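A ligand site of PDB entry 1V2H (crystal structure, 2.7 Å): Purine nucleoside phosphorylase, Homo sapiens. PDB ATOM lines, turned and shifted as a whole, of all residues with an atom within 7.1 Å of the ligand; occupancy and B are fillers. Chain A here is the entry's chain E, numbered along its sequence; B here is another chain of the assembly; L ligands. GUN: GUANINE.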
ATOM      1  N   ASN A 114     -23.874 -28.336  35.274  1.00  0.00           N
ATOM      2  CA  ASN A 114     -23.400 -27.834  33.998  1.00  0.00           C
ATOM      3  C   ASN A 114     -22.094 -28.472  33.574  1.00  0.00           C
ATOM      4  O   ASN A 114     -21.517 -29.248  34.332  1.00  0.00           O
ATOM      5  CB  ASN A 114     -23.278 -26.305  34.020  1.00  0.00           C
ATOM      6  CG  ASN A 114     -22.243 -25.804  34.983  1.00  0.00           C
ATOM      7  OD1 ASN A 114     -22.549 -25.057  35.892  1.00  0.00           O
ATOM      8  ND2 ASN A 114     -21.007 -26.136  34.723  1.00  0.00           N
ATOM      9  N   ALA A 115     -21.689 -28.250  32.335  1.00  0.00           N
ATOM     10  CA  ALA A 115     -20.421 -28.757  31.843  1.00  0.00           C
ATOM     11  C   ALA A 115     -19.625 -27.494  31.712  1.00  0.00           C
ATOM     12  O   ALA A 115     -20.180 -26.457  31.383  1.00  0.00           O
ATOM     13  CB  ALA A 115     -20.585 -29.389  30.518  1.00  0.00           C
ATOM     14  N   ALA A 116     -18.337 -27.539  32.003  1.00  0.00           N
ATOM     15  CA  ALA A 116     -17.543 -26.335  31.947  1.00  0.00           C
ATOM     16  C   ALA A 116     -16.121 -26.672  31.549  1.00  0.00           C
ATOM     17  O   ALA A 116     -15.750 -27.837  31.570  1.00  0.00           O
ATOM     18  CB  ALA A 116     -17.560 -25.684  33.315  1.00  0.00           C
ATOM     19  N   GLY A 117     -15.347 -25.666  31.183  1.00  0.00           N
ATOM     20  CA  GLY A 117     -13.968 -25.867  30.793  1.00  0.00           C
ATOM     21  C   GLY A 117     -13.114 -25.610  32.016  1.00  0.00           C
ATOM     22  O   GLY A 117     -13.475 -24.772  32.836  1.00  0.00           O
ATOM     23  N   GLY A 118     -11.988 -26.296  32.130  1.00  0.00           N
ATOM     24  CA  GLY A 118     -11.107 -26.153  33.274  1.00  0.00           C
ATOM     25  C   GLY A 118     -10.126 -25.004  33.152  1.00  0.00           C
ATOM     26  O   GLY A 118      -9.322 -24.965  32.211  1.00  0.00           O
ATOM     27  N   TYR A 191     -17.059 -20.527  39.513  1.00  0.00           N
ATOM     28  CA  TYR A 191     -17.507 -20.716  38.147  1.00  0.00           C
ATOM     29  C   TYR A 191     -17.745 -19.331  37.503  1.00  0.00           C
ATOM     30  O   TYR A 191     -18.448 -18.482  38.069  1.00  0.00           O
ATOM     31  CB  TYR A 191     -18.804 -21.528  38.174  1.00  0.00           C
ATOM     32  CG  TYR A 191     -19.503 -21.642  36.846  1.00  0.00           C
ATOM     33  CD1 TYR A 191     -19.289 -22.749  36.022  1.00  0.00           C
ATOM     34  CD2 TYR A 191     -20.410 -20.675  36.434  1.00  0.00           C
ATOM     35  CE1 TYR A 191     -19.983 -22.881  34.829  1.00  0.00           C
ATOM     36  CE2 TYR A 191     -21.097 -20.800  35.231  1.00  0.00           C
ATOM     37  CZ  TYR A 191     -20.877 -21.913  34.435  1.00  0.00           C
ATOM     38  OH  TYR A 191     -21.573 -22.033  33.250  1.00  0.00           O
ATOM     39  N   VAL A 192     -17.180 -19.102  36.329  1.00  0.00           N
ATOM     40  CA  VAL A 192     -17.377 -17.827  35.646  1.00  0.00           C
ATOM     41  C   VAL A 192     -18.296 -18.022  34.453  1.00  0.00           C
ATOM     42  O   VAL A 192     -18.003 -18.862  33.589  1.00  0.00           O
ATOM     43  CB  VAL A 192     -16.017 -17.178  35.202  1.00  0.00           C
ATOM     44  CG1 VAL A 192     -15.216 -18.106  34.327  1.00  0.00           C
ATOM     45  CG2 VAL A 192     -16.264 -15.865  34.494  1.00  0.00           C
ATOM     46  N   VAL A 194     -19.909 -16.904  31.016  1.00  0.00           N
ATOM     47  CA  VAL A 194     -19.483 -16.153  29.849  1.00  0.00           C
ATOM     48  C   VAL A 194     -20.653 -16.430  28.914  1.00  0.00           C
ATOM     49  O   VAL A 194     -21.237 -17.494  28.975  1.00  0.00           O
ATOM     50  CB  VAL A 194     -18.167 -16.755  29.350  1.00  0.00           C
ATOM     51  CG1 VAL A 194     -18.194 -17.022  27.858  1.00  0.00           C
ATOM     52  CG2 VAL A 194     -17.017 -15.841  29.752  1.00  0.00           C
ATOM     53  N   ALA A 195     -21.019 -15.481  28.059  1.00  0.00           N
ATOM     54  CA  ALA A 195     -22.172 -15.715  27.212  1.00  0.00           C
ATOM     55  C   ALA A 195     -21.990 -16.417  25.883  1.00  0.00           C
ATOM     56  O   ALA A 195     -22.532 -17.495  25.692  1.00  0.00           O
ATOM     57  CB  ALA A 195     -22.920 -14.439  26.983  1.00  0.00           C
ATOM     58  N   GLY A 196     -21.360 -15.702  24.944  1.00  0.00           N
ATOM     59  CA  GLY A 196     -21.126 -16.122  23.568  1.00  0.00           C
ATOM     60  C   GLY A 196     -21.062 -17.603  23.358  1.00  0.00           C
ATOM     61  O   GLY A 196     -20.629 -18.306  24.277  1.00  0.00           O
ATOM     62  N   PRO A 197     -21.499 -18.124  22.188  1.00  0.00           N
ATOM     63  CA  PRO A 197     -21.470 -19.564  21.926  1.00  0.00           C
ATOM     64  C   PRO A 197     -20.100 -20.100  21.515  1.00  0.00           C
ATOM     65  O   PRO A 197     -19.782 -21.268  21.742  1.00  0.00           O
ATOM     66  CB  PRO A 197     -22.505 -19.736  20.830  1.00  0.00           C
ATOM     67  CG  PRO A 197     -22.413 -18.507  20.084  1.00  0.00           C
ATOM     68  CD  PRO A 197     -22.284 -17.434  21.157  1.00  0.00           C
ATOM     69  N   SER A 198     -19.246 -19.252  20.958  1.00  0.00           N
ATOM     70  CA  SER A 198     -17.951 -19.711  20.534  1.00  0.00           C
ATOM     71  C   SER A 198     -17.086 -19.912  21.772  1.00  0.00           C
ATOM     72  O   SER A 198     -17.437 -19.447  22.845  1.00  0.00           O
ATOM     73  CB  SER A 198     -17.351 -18.730  19.524  1.00  0.00           C
ATOM     74  OG  SER A 198     -17.364 -17.406  20.026  1.00  0.00           O
ATOM     75  N   PHE A 199     -16.018 -20.690  21.653  1.00  0.00           N
ATOM     76  CA  PHE A 199     -15.139 -20.945  22.787  1.00  0.00           C
ATOM     77  C   PHE A 199     -14.061 -19.882  22.889  1.00  0.00           C
ATOM     78  O   PHE A 199     -13.786 -19.139  21.939  1.00  0.00           O
ATOM     79  CB  PHE A 199     -14.541 -22.341  22.688  1.00  0.00           C
ATOM     80  CG  PHE A 199     -15.519 -23.456  22.940  1.00  0.00           C
ATOM     81  CD1 PHE A 199     -16.759 -23.202  23.510  1.00  0.00           C
ATOM     82  CD2 PHE A 199     -15.208 -24.755  22.613  1.00  0.00           C
ATOM     83  CE1 PHE A 199     -17.660 -24.223  23.748  1.00  0.00           C
ATOM     84  CE2 PHE A 199     -16.098 -25.789  22.849  1.00  0.00           C
ATOM     85  CZ  PHE A 199     -17.325 -25.517  23.420  1.00  0.00           C
ATOM     86  N   GLU A 200     -13.364 -19.847  24.008  1.00  0.00           N
ATOM     87  CA  GLU A 200     -12.372 -18.810  24.202  1.00  0.00           C
ATOM     88  C   GLU A 200     -10.978 -18.914  23.618  1.00  0.00           C
ATOM     89  O   GLU A 200     -10.414 -19.985  23.429  1.00  0.00           O
ATOM     90  CB  GLU A 200     -12.281 -18.383  25.679  1.00  0.00           C
ATOM     91  CG  GLU A 200     -12.513 -19.460  26.680  1.00  0.00           C
ATOM     92  CD  GLU A 200     -13.966 -19.758  26.870  1.00  0.00           C
ATOM     93  OE1 GLU A 200     -14.707 -18.855  27.286  1.00  0.00           O
ATOM     94  OE2 GLU A 200     -14.361 -20.905  26.599  1.00  0.00           O
ATOM     95  N   CYS A 205      -8.849 -16.925  27.820  1.00  0.00           N
ATOM     96  CA  CYS A 205      -8.655 -17.941  28.829  1.00  0.00           C
ATOM     97  C   CYS A 205      -7.805 -17.405  29.979  1.00  0.00           C
ATOM     98  O   CYS A 205      -7.963 -17.829  31.112  1.00  0.00           O
ATOM     99  CB  CYS A 205      -7.962 -19.151  28.215  1.00  0.00           C
ATOM    100  SG  CYS A 205      -8.576 -20.692  28.877  1.00  0.00           S
ATOM    101  N   LEU A 208      -9.946 -14.663  32.425  1.00  0.00           N
ATOM    102  CA  LEU A 208     -10.825 -15.432  33.326  1.00  0.00           C
ATOM    103  C   LEU A 208      -9.991 -16.074  34.448  1.00  0.00           C
ATOM    104  O   LEU A 208     -10.445 -16.138  35.582  1.00  0.00           O
ATOM    105  CB  LEU A 208     -11.567 -16.520  32.543  1.00  0.00           C
ATOM    106  CG  LEU A 208     -12.779 -16.160  31.676  1.00  0.00           C
ATOM    107  CD1 LEU A 208     -12.981 -14.691  31.648  1.00  0.00           C
ATOM    108  CD2 LEU A 208     -12.627 -16.720  30.289  1.00  0.00           C
ATOM    109  N   VAL A 216     -15.080 -22.277  33.403  1.00  0.00           N
ATOM    110  CA  VAL A 216     -15.901 -21.323  32.634  1.00  0.00           C
ATOM    111  C   VAL A 216     -17.094 -22.016  31.961  1.00  0.00           C
ATOM    112  O   VAL A 216     -16.989 -23.159  31.544  1.00  0.00           O
ATOM    113  CB  VAL A 216     -15.036 -20.535  31.592  1.00  0.00           C
ATOM    114  CG1 VAL A 216     -14.286 -21.472  30.660  1.00  0.00           C
ATOM    115  CG2 VAL A 216     -15.901 -19.549  30.826  1.00  0.00           C
ATOM    116  N   GLY A 217     -18.227 -21.347  31.918  1.00  0.00           N
ATOM    117  CA  GLY A 217     -19.397 -21.968  31.327  1.00  0.00           C
ATOM    118  C   GLY A 217     -20.308 -20.916  30.750  1.00  0.00           C
ATOM    119  O   GLY A 217     -19.982 -19.738  30.816  1.00  0.00           O
ATOM    120  N   MET A 218     -21.470 -21.322  30.261  1.00  0.00           N
ATOM    121  CA  MET A 218     -22.389 -20.394  29.624  1.00  0.00           C
ATOM    122  C   MET A 218     -23.822 -20.435  30.163  1.00  0.00           C
ATOM    123  O   MET A 218     -24.743 -19.977  29.456  1.00  0.00           O
ATOM    124  CB  MET A 218     -22.417 -20.692  28.129  1.00  0.00           C
ATOM    125  CG  MET A 218     -21.081 -20.597  27.422  1.00  0.00           C
ATOM    126  SD  MET A 218     -21.196 -21.128  25.688  1.00  0.00           S
ATOM    127  CE  MET A 218     -19.445 -21.522  25.389  1.00  0.00           C
ATOM    128  N   LEU A 239     -19.288 -30.383  35.540  1.00  0.00           N
ATOM    129  CA  LEU A 239     -18.546 -31.524  35.022  1.00  0.00           C
ATOM    130  C   LEU A 239     -17.441 -30.957  34.096  1.00  0.00           C
ATOM    131  O   LEU A 239     -17.723 -30.513  32.981  1.00  0.00           O
ATOM    132  CB  LEU A 239     -19.481 -32.454  34.235  1.00  0.00           C
ATOM    133  CG  LEU A 239     -18.835 -33.626  33.482  1.00  0.00           C
ATOM    134  CD1 LEU A 239     -18.086 -34.467  34.437  1.00  0.00           C
ATOM    135  CD2 LEU A 239     -19.887 -34.449  32.791  1.00  0.00           C
ATOM    136  N   ILE A 240     -16.197 -30.905  34.579  1.00  0.00           N
ATOM    137  CA  ILE A 240     -15.108 -30.377  33.761  1.00  0.00           C
ATOM    138  C   ILE A 240     -14.971 -31.251  32.518  1.00  0.00           C
ATOM    139  O   ILE A 240     -14.464 -32.357  32.577  1.00  0.00           O
ATOM    140  CB  ILE A 240     -13.788 -30.389  34.555  1.00  0.00           C
ATOM    141  CG1 ILE A 240     -13.970 -29.665  35.889  1.00  0.00           C
ATOM    142  CG2 ILE A 240     -12.653 -29.753  33.762  1.00  0.00           C
ATOM    143  CD1 ILE A 240     -14.549 -28.274  35.757  1.00  0.00           C
ATOM    144  N   THR A 241     -15.479 -30.768  31.385  1.00  0.00           N
ATOM    145  CA  THR A 241     -15.411 -31.502  30.136  1.00  0.00           C
ATOM    146  C   THR A 241     -14.151 -31.233  29.316  1.00  0.00           C
ATOM    147  O   THR A 241     -13.927 -31.869  28.289  1.00  0.00           O
ATOM    148  CB  THR A 241     -16.602 -31.173  29.241  1.00  0.00           C
ATOM    149  OG1 THR A 241     -16.615 -29.780  28.926  1.00  0.00           O
ATOM    150  CG2 THR A 241     -17.879 -31.473  29.934  1.00  0.00           C
ATOM    151  N   ASN A 242     -13.334 -30.271  29.735  1.00  0.00           N
ATOM    152  CA  ASN A 242     -12.124 -29.904  28.989  1.00  0.00           C
ATOM    153  C   ASN A 242     -11.310 -28.849  29.737  1.00  0.00           C
ATOM    154  O   ASN A 242     -11.553 -28.620  30.911  1.00  0.00           O
ATOM    155  CB  ASN A 242     -12.485 -29.425  27.561  1.00  0.00           C
ATOM    156  CG  ASN A 242     -13.460 -28.235  27.545  1.00  0.00           C
ATOM    157  OD1 ASN A 242     -14.567 -28.318  28.038  1.00  0.00           O
ATOM    158  ND2 ASN A 242     -13.036 -27.145  26.912  1.00  0.00           N
ATOM    159  N   LYS A 243     -10.331 -28.217  29.063  1.00  0.00           N
ATOM    160  CA  LYS A 243      -9.493 -27.190  29.693  1.00  0.00           C
ATOM    161  C   LYS A 243      -8.449 -26.615  28.734  1.00  0.00           C
ATOM    162  O   LYS A 243      -7.913 -27.387  27.923  1.00  0.00           O
ATOM    163  CB  LYS A 243      -8.783 -27.824  30.878  1.00  0.00           C
ATOM    164  CG  LYS A 243      -7.970 -29.073  30.542  1.00  0.00           C
ATOM    165  CD  LYS A 243      -7.491 -29.826  31.811  1.00  0.00           C
ATOM    166  CE  LYS A 243      -6.746 -28.938  32.816  1.00  0.00           C
ATOM    167  NZ  LYS A 243      -7.663 -28.173  33.740  1.00  0.00           N
ATOM    168  N   VAL A 244      -8.155 -25.297  28.788  1.00  0.00           N
ATOM    169  CA  VAL A 244      -7.106 -24.665  27.919  1.00  0.00           C
ATOM    170  C   VAL A 244      -6.586 -23.311  28.455  1.00  0.00           C
ATOM    171  O   VAL A 244      -7.203 -22.764  29.362  1.00  0.00           O
ATOM    172  CB  VAL A 244      -7.576 -24.432  26.440  1.00  0.00           C
ATOM    173  CG1 VAL A 244      -8.593 -23.274  26.367  1.00  0.00           C
ATOM    174  CG2 VAL A 244      -6.352 -24.156  25.498  1.00  0.00           C
ATOM    175  N   ALA A 254     -10.228 -27.443  20.955  1.00  0.00           N
ATOM    176  CA  ALA A 254     -11.601 -27.781  21.370  1.00  0.00           C
ATOM    177  C   ALA A 254     -12.639 -27.556  20.270  1.00  0.00           C
ATOM    178  O   ALA A 254     -12.331 -27.008  19.209  1.00  0.00           O
ATOM    179  CB  ALA A 254     -12.002 -27.038  22.648  1.00  0.00           C
ATOM    180  N   GLU A 258     -15.105 -32.850  22.191  1.00  0.00           N
ATOM    181  CA  GLU A 258     -14.196 -32.788  23.326  1.00  0.00           C
ATOM    182  C   GLU A 258     -15.005 -32.640  24.602  1.00  0.00           C
ATOM    183  O   GLU A 258     -14.665 -33.227  25.637  1.00  0.00           O
ATOM    184  CB  GLU A 258     -13.232 -31.597  23.184  1.00  0.00           C
ATOM    185  CG  GLU A 258     -13.845 -30.290  22.666  1.00  0.00           C
ATOM    186  CD  GLU A 258     -14.746 -29.546  23.663  1.00  0.00           C
ATOM    187  OE1 GLU A 258     -14.546 -29.671  24.883  1.00  0.00           O
ATOM    188  OE2 GLU A 258     -15.653 -28.827  23.209  1.00  0.00           O
ATOM    189  N   VAL A 259     -16.064 -31.828  24.519  1.00  0.00           N
ATOM    190  CA  VAL A 259     -16.935 -31.604  25.673  1.00  0.00           C
ATOM    191  C   VAL A 259     -17.857 -32.815  25.818  1.00  0.00           C
ATOM    192  O   VAL A 259     -19.017 -32.837  25.378  1.00  0.00           O
ATOM    193  CB  VAL A 259     -17.700 -30.220  25.611  1.00  0.00           C
ATOM    194  CG1 VAL A 259     -18.450 -30.066  24.317  1.00  0.00           C
ATOM    195  CG2 VAL A 259     -18.659 -30.078  26.780  1.00  0.00           C
ATOM    196  N   PHE B 158     -20.649 -24.284  18.641  1.00  0.00           N
ATOM    197  CA  PHE B 158     -19.555 -23.810  19.468  1.00  0.00           C
ATOM    198  C   PHE B 158     -18.195 -23.754  18.750  1.00  0.00           C
ATOM    199  O   PHE B 158     -17.317 -24.593  18.972  1.00  0.00           O
ATOM    200  CB  PHE B 158     -19.448 -24.668  20.722  1.00  0.00           C
ATOM    201  CG  PHE B 158     -20.728 -24.856  21.450  1.00  0.00           C
ATOM    202  CD1 PHE B 158     -21.356 -23.788  22.057  1.00  0.00           C
ATOM    203  CD2 PHE B 158     -21.321 -26.102  21.526  1.00  0.00           C
ATOM    204  CE1 PHE B 158     -22.545 -23.966  22.723  1.00  0.00           C
ATOM    205  CE2 PHE B 158     -22.499 -26.294  22.189  1.00  0.00           C
ATOM    206  CZ  PHE B 158     -23.121 -25.219  22.787  1.00  0.00           C
HETATM  207  N9  GUN L   1     -18.331 -25.538  28.423  1.00  0.00           N
HETATM  208  C8  GUN L   1     -17.524 -26.700  28.440  1.00  0.00           C
HETATM  209  N7  GUN L   1     -16.233 -26.443  28.159  1.00  0.00           N
HETATM  210  C5  GUN L   1     -16.229 -25.045  27.943  1.00  0.00           C
HETATM  211  C6  GUN L   1     -15.157 -24.216  27.615  1.00  0.00           C
HETATM  212  O6  GUN L   1     -13.977 -24.540  27.440  1.00  0.00           O
HETATM  213  N1  GUN L   1     -15.538 -22.881  27.481  1.00  0.00           N
HETATM  214  C2  GUN L   1     -16.794 -22.446  27.655  1.00  0.00           C
HETATM  215  N2  GUN L   1     -17.010 -21.145  27.485  1.00  0.00           N
HETATM  216  N3  GUN L   1     -17.798 -23.224  27.954  1.00  0.00           N
HETATM  217  C4  GUN L   1     -17.468 -24.494  28.090  1.00  0.00           C
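N of Met 218 lies within hydrogen-bond range of OH of Tyr 191.
The backbone carbonyl oxygen (O) of Gly 217 sits at hydrogen-bond distance from the backbone NH (N) of Val 194, at 2.8 Å.
N of Gly 217 lies within hydrogen-bond range of O of Val 192, 3.0 Å away.
OD1 of Asn 242 lies close to OE1 of Glu 258 (3.4 Å).
The backbone carbonyl oxygen (O) of Val 216 sits at hydrogen-bond distance from the backbone NH (N) of Gly 117, at 3.0 Å.
The backbone NH (N) of Gly 118 lies within hydrogen-bond range of the backbone carbonyl oxygen (O) of Asn 242 (2.7 Å).
The backbone NH of Thr 241 sits at hydrogen-bond distance from the backbone carbonyl oxygen of Ala 116, 2.9 Å away.
O of Leu 239 sits at hydrogen-bond distance from N of Ala 116 (3.2 Å).
O of Ala 115 touches N9 of the ligand, at 3.6 Å.
C of Ala 116 touches N7 of the ligand, 3.4 Å away.
O of Val 216 touches N3 of the ligand, at 3.7 Å.
Gly 217 touches the ligand.
CE of Met 218 touches N2 of the ligand, 3.2 Å away.
Val 259 touches the ligand (CG2 to C8, 3.9 Å).
Of the 29 residues printed, 10 come within 4 Å of the ligand.
Along chain A the residues within 4 Å of the ligand span positions 115 to 259.
The nearest printed residue that does not touch the ligand is Phe 199 (4.2 Å).
The side-chain amide oxygen (OD1) of Asn 242 lies close to a nitrogen (N7) of the ligand, 2.5 Å away.
A nitrogen (N7) of the ligand sits close to the side-chain hydroxyl (OG1) of Thr 241, at 3.4 Å.
N7 of the ligand is in hydrogen-bond range of N of Gly 117.
OE2 of Glu 200 lies within hydrogen-bond range of N1 of the ligand.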
